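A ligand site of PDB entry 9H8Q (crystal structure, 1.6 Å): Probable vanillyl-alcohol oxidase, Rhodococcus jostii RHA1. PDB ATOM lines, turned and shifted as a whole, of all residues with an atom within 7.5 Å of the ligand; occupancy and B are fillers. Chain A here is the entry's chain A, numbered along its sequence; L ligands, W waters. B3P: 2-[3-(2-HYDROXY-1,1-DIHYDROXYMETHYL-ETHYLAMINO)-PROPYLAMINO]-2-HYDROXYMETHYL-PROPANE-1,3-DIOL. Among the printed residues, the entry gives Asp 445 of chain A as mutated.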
ATOM      1  N   ALA A  34     -12.586  40.956 -15.390  1.00  0.00           N
ATOM      2  CA  ALA A  34     -13.444  39.854 -15.799  1.00  0.00           C
ATOM      3  C   ALA A  34     -13.734  39.925 -17.291  1.00  0.00           C
ATOM      4  O   ALA A  34     -13.626  38.930 -17.993  1.00  0.00           O
ATOM      5  CB  ALA A  34     -14.724  39.871 -14.997  1.00  0.00           C
ATOM      6  N   LEU A  37     -10.797  39.094 -19.545  1.00  0.00           N
ATOM      7  CA  LEU A  37     -10.386  37.702 -19.479  1.00  0.00           C
ATOM      8  C   LEU A  37     -11.365  36.789 -20.227  1.00  0.00           C
ATOM      9  O   LEU A  37     -11.038  35.675 -20.526  1.00  0.00           O
ATOM     10  CB  LEU A  37     -10.222  37.277 -18.025  1.00  0.00           C
ATOM     11  CG  LEU A  37      -9.101  37.995 -17.266  1.00  0.00           C
ATOM     12  CD1 LEU A  37      -9.118  37.665 -15.817  1.00  0.00           C
ATOM     13  CD2 LEU A  37      -7.760  37.592 -17.788  1.00  0.00           C
ATOM     14  N   GLU A  38     -12.577  37.261 -20.505  1.00  0.00           N
ATOM     15  CA  GLU A  38     -13.608  36.452 -21.141  1.00  0.00           C
ATOM     16  C   GLU A  38     -13.117  35.858 -22.447  1.00  0.00           C
ATOM     17  O   GLU A  38     -13.405  34.672 -22.712  1.00  0.00           O
ATOM     18  CB  GLU A  38     -14.844  37.337 -21.380  1.00  0.00           C
ATOM     19  CG  GLU A  38     -16.032  36.608 -21.975  1.00  0.00           C
ATOM     20  CD  GLU A  38     -16.647  35.559 -21.068  1.00  0.00           C
ATOM     21  OE1 GLU A  38     -16.424  35.517 -19.826  1.00  0.00           O
ATOM     22  OE2 GLU A  38     -17.323  34.716 -21.695  1.00  0.00           O
ATOM     23  N   ALA A  39     -12.321  36.624 -23.206  1.00  0.00           N
ATOM     24  CA  ALA A  39     -11.873  36.139 -24.509  1.00  0.00           C
ATOM     25  C   ALA A  39     -10.797  35.063 -24.375  1.00  0.00           C
ATOM     26  O   ALA A  39     -10.393  34.462 -25.369  1.00  0.00           O
ATOM     27  CB  ALA A  39     -11.380  37.290 -25.362  1.00  0.00           C
ATOM     28  N   ARG A  41     -11.078  32.594 -21.978  1.00  0.00           N
ATOM     29  CA  ARG A  41     -11.708  31.381 -21.484  1.00  0.00           C
ATOM     30  C   ARG A  41     -11.766  30.445 -22.693  1.00  0.00           C
ATOM     31  O   ARG A  41     -11.738  30.885 -23.858  1.00  0.00           O
ATOM     32  CB  ARG A  41     -13.088  31.655 -20.902  1.00  0.00           C
ATOM     33  CG  ARG A  41     -13.034  32.352 -19.551  1.00  0.00           C
ATOM     34  CD  ARG A  41     -14.415  32.544 -18.978  1.00  0.00           C
ATOM     35  NE  ARG A  41     -14.399  33.068 -17.610  1.00  0.00           N
ATOM     36  CZ  ARG A  41     -15.407  32.957 -16.739  1.00  0.00           C
ATOM     37  NH1 ARG A  41     -16.482  32.231 -17.023  1.00  0.00           N
ATOM     38  NH2 ARG A  41     -15.255  33.481 -15.524  1.00  0.00           N
ATOM     39  N   ASP A  42     -11.814  29.140 -22.411  1.00  0.00           N
ATOM     40  CA  ASP A  42     -12.000  28.159 -23.460  1.00  0.00           C
ATOM     41  C   ASP A  42     -13.222  28.527 -24.296  1.00  0.00           C
ATOM     42  O   ASP A  42     -14.321  28.604 -23.755  1.00  0.00           O
ATOM     43  CB  ASP A  42     -12.112  26.787 -22.827  1.00  0.00           C
ATOM     44  CG  ASP A  42     -12.144  25.596 -23.784  1.00  0.00           C
ATOM     45  OD1 ASP A  42     -12.229  25.801 -25.010  1.00  0.00           O
ATOM     46  OD2 ASP A  42     -12.059  24.491 -23.283  1.00  0.00           O
ATOM     47  N   PRO A  43     -13.111  28.737 -25.617  1.00  0.00           N
ATOM     48  CA  PRO A  43     -14.303  29.034 -26.419  1.00  0.00           C
ATOM     49  C   PRO A  43     -15.244  27.853 -26.555  1.00  0.00           C
ATOM     50  O   PRO A  43     -16.430  28.046 -26.813  1.00  0.00           O
ATOM     51  CB  PRO A  43     -13.735  29.469 -27.745  1.00  0.00           C
ATOM     52  CG  PRO A  43     -12.423  28.729 -27.861  1.00  0.00           C
ATOM     53  CD  PRO A  43     -11.887  28.667 -26.434  1.00  0.00           C
ATOM     54  N   TYR A  44     -14.717  26.644 -26.376  1.00  0.00           N
ATOM     55  CA  TYR A  44     -15.466  25.398 -26.531  1.00  0.00           C
ATOM     56  C   TYR A  44     -15.433  24.658 -25.200  1.00  0.00           C
ATOM     57  O   TYR A  44     -14.744  23.650 -25.059  1.00  0.00           O
ATOM     58  CB  TYR A  44     -14.903  24.547 -27.662  1.00  0.00           C
ATOM     59  CG  TYR A  44     -14.768  25.211 -29.028  1.00  0.00           C
ATOM     60  CD1 TYR A  44     -15.515  26.321 -29.413  1.00  0.00           C
ATOM     61  CD2 TYR A  44     -13.826  24.735 -29.937  1.00  0.00           C
ATOM     62  CE1 TYR A  44     -15.371  26.895 -30.665  1.00  0.00           C
ATOM     63  CE2 TYR A  44     -13.671  25.313 -31.182  1.00  0.00           C
ATOM     64  CZ  TYR A  44     -14.436  26.401 -31.551  1.00  0.00           C
ATOM     65  OH  TYR A  44     -14.265  26.961 -32.793  1.00  0.00           O
ATOM     66  N   PRO A  45     -16.077  25.196 -24.140  1.00  0.00           N
ATOM     67  CA  PRO A  45     -15.950  24.647 -22.797  1.00  0.00           C
ATOM     68  C   PRO A  45     -16.512  23.238 -22.716  1.00  0.00           C
ATOM     69  O   PRO A  45     -17.508  22.919 -23.394  1.00  0.00           O
ATOM     70  CB  PRO A  45     -16.748  25.631 -21.937  1.00  0.00           C
ATOM     71  CG  PRO A  45     -17.734  26.256 -22.902  1.00  0.00           C
ATOM     72  CD  PRO A  45     -16.930  26.394 -24.163  1.00  0.00           C
ATOM     73  N   GLY A  47     -17.739  20.340 -19.799  1.00  0.00           N
ATOM     74  CA  GLY A  47     -18.269  20.277 -18.448  1.00  0.00           C
ATOM     75  C   GLY A  47     -19.201  21.448 -18.183  1.00  0.00           C
ATOM     76  O   GLY A  47     -18.984  22.553 -18.703  1.00  0.00           O
ATOM     77  N   ALA A  48     -20.251  21.204 -17.394  1.00  0.00           N
ATOM     78  CA  ALA A  48     -21.196  22.268 -17.071  1.00  0.00           C
ATOM     79  C   ALA A  48     -20.522  23.292 -16.149  1.00  0.00           C
ATOM     80  O   ALA A  48     -20.722  24.488 -16.287  1.00  0.00           O
ATOM     81  CB  ALA A  48     -22.438  21.701 -16.440  1.00  0.00           C
ATOM     82  N   ALA A  49     -19.782  22.804 -15.139  1.00  0.00           N
ATOM     83  CA  ALA A  49     -19.182  23.688 -14.149  1.00  0.00           C
ATOM     84  C   ALA A  49     -18.028  24.464 -14.792  1.00  0.00           C
ATOM     85  O   ALA A  49     -17.368  23.979 -15.708  1.00  0.00           O
ATOM     86  CB  ALA A  49     -18.672  22.904 -12.961  1.00  0.00           C
ATOM     87  N   GLU A  50     -17.789  25.679 -14.304  1.00  0.00           N
ATOM     88  CA  GLU A  50     -16.691  26.475 -14.808  1.00  0.00           C
ATOM     89  C   GLU A  50     -15.388  25.789 -14.446  1.00  0.00           C
ATOM     90  O   GLU A  50     -15.256  25.146 -13.397  1.00  0.00           O
ATOM     91  CB  GLU A  50     -16.758  27.909 -14.284  1.00  0.00           C
ATOM     92  CG  GLU A  50     -17.817  28.754 -14.983  1.00  0.00           C
ATOM     93  CD  GLU A  50     -17.633  28.879 -16.497  1.00  0.00           C
ATOM     94  OE1 GLU A  50     -16.744  28.217 -17.088  1.00  0.00           O
ATOM     95  OE2 GLU A  50     -18.421  29.642 -17.069  1.00  0.00           O
ATOM     96  N   ALA A  51     -14.432  25.886 -15.367  1.00  0.00           N
ATOM     97  CA  ALA A  51     -13.112  25.302 -15.141  1.00  0.00           C
ATOM     98  C   ALA A  51     -12.110  26.078 -15.989  1.00  0.00           C
ATOM     99  O   ALA A  51     -12.501  26.839 -16.884  1.00  0.00           O
ATOM    100  CB  ALA A  51     -13.155  23.845 -15.523  1.00  0.00           C
ATOM    101  N   LEU A  53      -9.978  28.579 -15.487  1.00  0.00           N
ATOM    102  CA  LEU A  53     -10.176  30.011 -15.467  1.00  0.00           C
ATOM    103  C   LEU A  53      -8.838  30.717 -15.314  1.00  0.00           C
ATOM    104  O   LEU A  53      -8.121  30.474 -14.349  1.00  0.00           O
ATOM    105  CB  LEU A  53     -11.102  30.382 -14.313  1.00  0.00           C
ATOM    106  CG  LEU A  53     -12.516  29.831 -14.412  1.00  0.00           C
ATOM    107  CD1 LEU A  53     -13.447  30.379 -13.384  1.00  0.00           C
ATOM    108  CD2 LEU A  53     -13.158  30.095 -15.772  1.00  0.00           C
ATOM    109  N   LEU A 382     -18.381  24.678 -37.298  1.00  0.00           N
ATOM    110  CA  LEU A 382     -18.981  25.054 -36.027  1.00  0.00           C
ATOM    111  C   LEU A 382     -20.403  25.589 -36.178  1.00  0.00           C
ATOM    112  O   LEU A 382     -21.081  25.800 -35.186  1.00  0.00           O
ATOM    113  CB  LEU A 382     -18.104  26.085 -35.286  1.00  0.00           C
ATOM    114  CG  LEU A 382     -16.819  25.562 -34.633  1.00  0.00           C
ATOM    115  CD1 LEU A 382     -17.031  24.272 -33.879  1.00  0.00           C
ATOM    116  CD2 LEU A 382     -15.691  25.363 -35.620  1.00  0.00           C
ATOM    117  N   PRO A 386     -26.275  25.391 -33.214  1.00  0.00           N
ATOM    118  CA  PRO A 386     -26.126  26.721 -32.617  1.00  0.00           C
ATOM    119  C   PRO A 386     -25.026  26.795 -31.571  1.00  0.00           C
ATOM    120  O   PRO A 386     -24.816  25.826 -30.837  1.00  0.00           O
ATOM    121  CB  PRO A 386     -27.493  27.008 -32.022  1.00  0.00           C
ATOM    122  CG  PRO A 386     -28.433  26.080 -32.795  1.00  0.00           C
ATOM    123  CD  PRO A 386     -27.632  24.842 -33.068  1.00  0.00           C
ATOM    124  N   ASN A 387     -24.319  27.932 -31.544  1.00  0.00           N
ATOM    125  CA  ASN A 387     -23.270  28.182 -30.562  1.00  0.00           C
ATOM    126  C   ASN A 387     -22.213  27.065 -30.602  1.00  0.00           C
ATOM    127  O   ASN A 387     -21.715  26.612 -29.569  1.00  0.00           O
ATOM    128  CB  ASN A 387     -23.844  28.308 -29.161  1.00  0.00           C
ATOM    129  CG  ASN A 387     -25.065  29.205 -29.122  1.00  0.00           C
ATOM    130  OD1 ASN A 387     -24.978  30.383 -29.435  1.00  0.00           O
ATOM    131  ND2 ASN A 387     -26.213  28.650 -28.748  1.00  0.00           N
ATOM    132  N   GLY A 388     -21.905  26.624 -31.822  1.00  0.00           N
ATOM    133  CA  GLY A 388     -21.120  25.420 -32.036  1.00  0.00           C
ATOM    134  C   GLY A 388     -19.707  25.525 -31.464  1.00  0.00           C
ATOM    135  O   GLY A 388     -19.043  26.543 -31.585  1.00  0.00           O
ATOM    136  N   GLY A 389     -19.304  24.450 -30.780  1.00  0.00           N
ATOM    137  CA  GLY A 389     -17.928  24.185 -30.384  1.00  0.00           C
ATOM    138  C   GLY A 389     -17.579  22.740 -30.677  1.00  0.00           C
ATOM    139  O   GLY A 389     -18.461  21.945 -31.010  1.00  0.00           O
ATOM    140  N   TYR A 441     -21.012  20.535 -30.596  1.00  0.00           N
ATOM    141  CA  TYR A 441     -22.075  20.635 -29.600  1.00  0.00           C
ATOM    142  C   TYR A 441     -22.378  22.097 -29.308  1.00  0.00           C
ATOM    143  O   TYR A 441     -21.600  22.974 -29.677  1.00  0.00           O
ATOM    144  CB  TYR A 441     -21.697  19.849 -28.322  1.00  0.00           C
ATOM    145  CG  TYR A 441     -20.474  20.424 -27.639  1.00  0.00           C
ATOM    146  CD1 TYR A 441     -19.209  20.139 -28.109  1.00  0.00           C
ATOM    147  CD2 TYR A 441     -20.596  21.345 -26.591  1.00  0.00           C
ATOM    148  CE1 TYR A 441     -18.077  20.694 -27.540  1.00  0.00           C
ATOM    149  CE2 TYR A 441     -19.476  21.899 -26.001  1.00  0.00           C
ATOM    150  CZ  TYR A 441     -18.218  21.618 -26.507  1.00  0.00           C
ATOM    151  OH  TYR A 441     -17.103  22.149 -25.936  1.00  0.00           O
ATOM    152  N   ASP A 442     -23.532  22.338 -28.664  1.00  0.00           N
ATOM    153  CA  ASP A 442     -23.971  23.672 -28.287  1.00  0.00           C
ATOM    154  C   ASP A 442     -23.262  24.119 -27.015  1.00  0.00           C
ATOM    155  O   ASP A 442     -23.588  23.670 -25.937  1.00  0.00           O
ATOM    156  CB  ASP A 442     -25.486  23.680 -28.149  1.00  0.00           C
ATOM    157  CG  ASP A 442     -26.123  25.032 -27.837  1.00  0.00           C
ATOM    158  OD1 ASP A 442     -25.406  25.953 -27.471  1.00  0.00           O
ATOM    159  OD2 ASP A 442     -27.346  25.151 -28.007  1.00  0.00           O
ATOM    160  N   THR A 443     -22.285  25.024 -27.145  1.00  0.00           N
ATOM    161  CA  THR A 443     -21.474  25.466 -26.012  1.00  0.00           C
ATOM    162  C   THR A 443     -22.282  26.303 -25.008  1.00  0.00           C
ATOM    163  O   THR A 443     -21.800  26.525 -23.897  1.00  0.00           O
ATOM    164  CB  THR A 443     -20.267  26.286 -26.495  1.00  0.00           C
ATOM    165  OG1 THR A 443     -20.714  27.474 -27.147  1.00  0.00           O
ATOM    166  CG2 THR A 443     -19.358  25.498 -27.424  1.00  0.00           C
ATOM    167  N   ALA A 444     -23.482  26.760 -25.370  1.00  0.00           N
ATOM    168  CA  ALA A 444     -24.288  27.572 -24.484  1.00  0.00           C
ATOM    169  C   ALA A 444     -25.183  26.703 -23.598  1.00  0.00           C
ATOM    170  O   ALA A 444     -25.852  27.224 -22.708  1.00  0.00           O
ATOM    171  CB  ALA A 444     -25.135  28.550 -25.282  1.00  0.00           C
ATOM    172  N   ASP A 445     -25.236  25.391 -23.866  1.00  0.00           N
ATOM    173  CA  ASP A 445     -26.130  24.482 -23.160  1.00  0.00           C
ATOM    174  C   ASP A 445     -25.326  23.716 -22.093  1.00  0.00           C
ATOM    175  O   ASP A 445     -24.492  22.880 -22.446  1.00  0.00           O
ATOM    176  CB  ASP A 445     -26.778  23.537 -24.157  1.00  0.00           C
ATOM    177  CG  ASP A 445     -27.745  22.521 -23.574  1.00  0.00           C
ATOM    178  OD1 ASP A 445     -27.840  22.422 -22.332  1.00  0.00           O
ATOM    179  OD2 ASP A 445     -28.391  21.816 -24.384  1.00  0.00           O
ATOM    180  N   ARG A 449     -22.591  20.549 -22.554  1.00  0.00           N
ATOM    181  CA  ARG A 449     -21.214  20.652 -22.069  1.00  0.00           C
ATOM    182  C   ARG A 449     -20.881  19.457 -21.162  1.00  0.00           C
ATOM    183  O   ARG A 449     -19.797  18.875 -21.250  1.00  0.00           O
ATOM    184  CB  ARG A 449     -20.949  21.956 -21.308  1.00  0.00           C
ATOM    185  CG  ARG A 449     -21.007  23.171 -22.202  1.00  0.00           C
ATOM    186  CD  ARG A 449     -20.622  24.484 -21.503  1.00  0.00           C
ATOM    187  NE  ARG A 449     -19.948  24.542 -20.218  1.00  0.00           N
ATOM    188  CZ  ARG A 449     -19.406  25.661 -19.692  1.00  0.00           C
ATOM    189  NH1 ARG A 449     -19.740  26.860 -20.142  1.00  0.00           N
ATOM    190  NH2 ARG A 449     -18.636  25.566 -18.618  1.00  0.00           N
HETATM  191  C1  B3P L   1     -19.003  29.311 -24.475  1.00  0.00           C
HETATM  192  C2  B3P L   1     -19.404  29.969 -23.160  1.00  0.00           C
HETATM  193  C3  B3P L   1     -18.734  30.296 -25.597  1.00  0.00           C
HETATM  194  N1  B3P L   1     -18.601  29.682 -26.926  1.00  0.00           N
HETATM  195  C4  B3P L   1     -18.665  30.576 -28.117  1.00  0.00           C
HETATM  196  C5  B3P L   1     -19.997  31.336 -28.219  1.00  0.00           C
HETATM  197  C6  B3P L   1     -18.483  29.707 -29.364  1.00  0.00           C
HETATM  198  C7  B3P L   1     -17.565  31.654 -28.126  1.00  0.00           C
HETATM  199  N2  B3P L   1     -18.240  30.494 -22.429  1.00  0.00           N
HETATM  200  C8  B3P L   1     -18.521  31.393 -21.275  1.00  0.00           C
HETATM  201  C9  B3P L   1     -17.187  31.982 -20.791  1.00  0.00           C
HETATM  202  C10 B3P L   1     -19.194  30.607 -20.130  1.00  0.00           C
HETATM  203  C11 B3P L   1     -19.430  32.540 -21.728  1.00  0.00           C
HETATM  204  O1  B3P L   1     -17.366  33.011 -19.832  1.00  0.00           O
HETATM  205  O2  B3P L   1     -18.435  29.477 -19.705  1.00  0.00           O
HETATM  206  O3  B3P L   1     -18.964  33.122 -22.950  1.00  0.00           O
HETATM  207  O4  B3P L   1     -21.070  30.472 -28.476  1.00  0.00           O
HETATM  208  O5  B3P L   1     -18.412  30.530 -30.519  1.00  0.00           O
HETATM  209  O6  B3P L   1     -16.410  31.235 -27.421  1.00  0.00           O
HETATM  210  O   HOH W   1     -15.837  29.035 -21.670  1.00  0.00           O
HETATM  211  O   HOH W   2     -16.523  31.888 -24.038  1.00  0.00           O
HETATM  212  O   HOH W   3     -19.001  28.911 -32.617  1.00  0.00           O
HETATM  213  O   HOH W   4     -14.472  33.116 -27.193  1.00  0.00           O
HETATM  214  O   HOH W   5     -22.711  30.421 -22.278  1.00  0.00           O
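The guanidinium group (NE) of Arg 41 lies within salt-bridge range of the side-chain carboxylate (OE1) of Glu 38 (3.9 Å).
The side-chain carboxylate of Glu 50 is in salt-bridge range of the guanidinium group of Arg 449 (3.6 Å).
NH1 of Arg 41 lies within salt-bridge range of OE2 of Glu 50 (3.2 Å).
NH2 of Arg 449 sits at hydrogen-bond distance from O of Ala 48.
NE of Arg 449 lies within hydrogen-bond range of O of Gly 47, at 2.7 Å.
OG1 of Thr 443 is in hydrogen-bond range of O of Asn 387 (2.8 Å).
OD1 of Asp 442 is in hydrogen-bond range of ND2 of Asn 387, at 3.1 Å.
O of Pro 45 is in hydrogen-bond range of OH of Tyr 441 (2.7 Å).
Residues that only touch the ligand: Asn 387, Pro 45 and Gly 388.
Hydrophobic or aromatic side chains that line the ligand: Pro 43 and Pro 45.
Nine residues have an atom within 4 Å of the ligand: Glu 38, Arg 41, Pro 43, Pro 45, Glu 50, Asn 387, Gly 388, Thr 443 and Arg 449.
An oxygen (O1) of the ligand is in hydrogen-bond range of the side-chain carboxylate (OE2) of Glu 38 (2.5 Å).
An oxygen (O2) of the ligand lies within hydrogen-bond range of the side-chain carboxylate (OE2) of Glu 50 (2.6 Å).
The backbone carbonyl oxygen (O) of Pro 43 sits at hydrogen-bond distance from a nitrogen (N1) of the ligand, 2.7 Å away.
The guanidinium group (NH1) of Arg 449 is in hydrogen-bond range of an oxygen (O2) of the ligand, 3.0 Å away.
The guanidinium group (NH1) of Arg 41 lies within hydrogen-bond range of an oxygen (O1) of the ligand (3.0 Å).
The side-chain hydroxyl of Thr 443 is in hydrogen-bond range of a nitrogen (N1) of the ligand.
Water W3 bridges the backbone carbonyl oxygen of Gly 388 (2.6 Å) and an oxygen (O5) of the ligand (2.7 Å).
Water W1 lies within hydrogen-bond range of O of Asp 42 (2.6 Å) and N2 of the ligand (2.9 Å).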
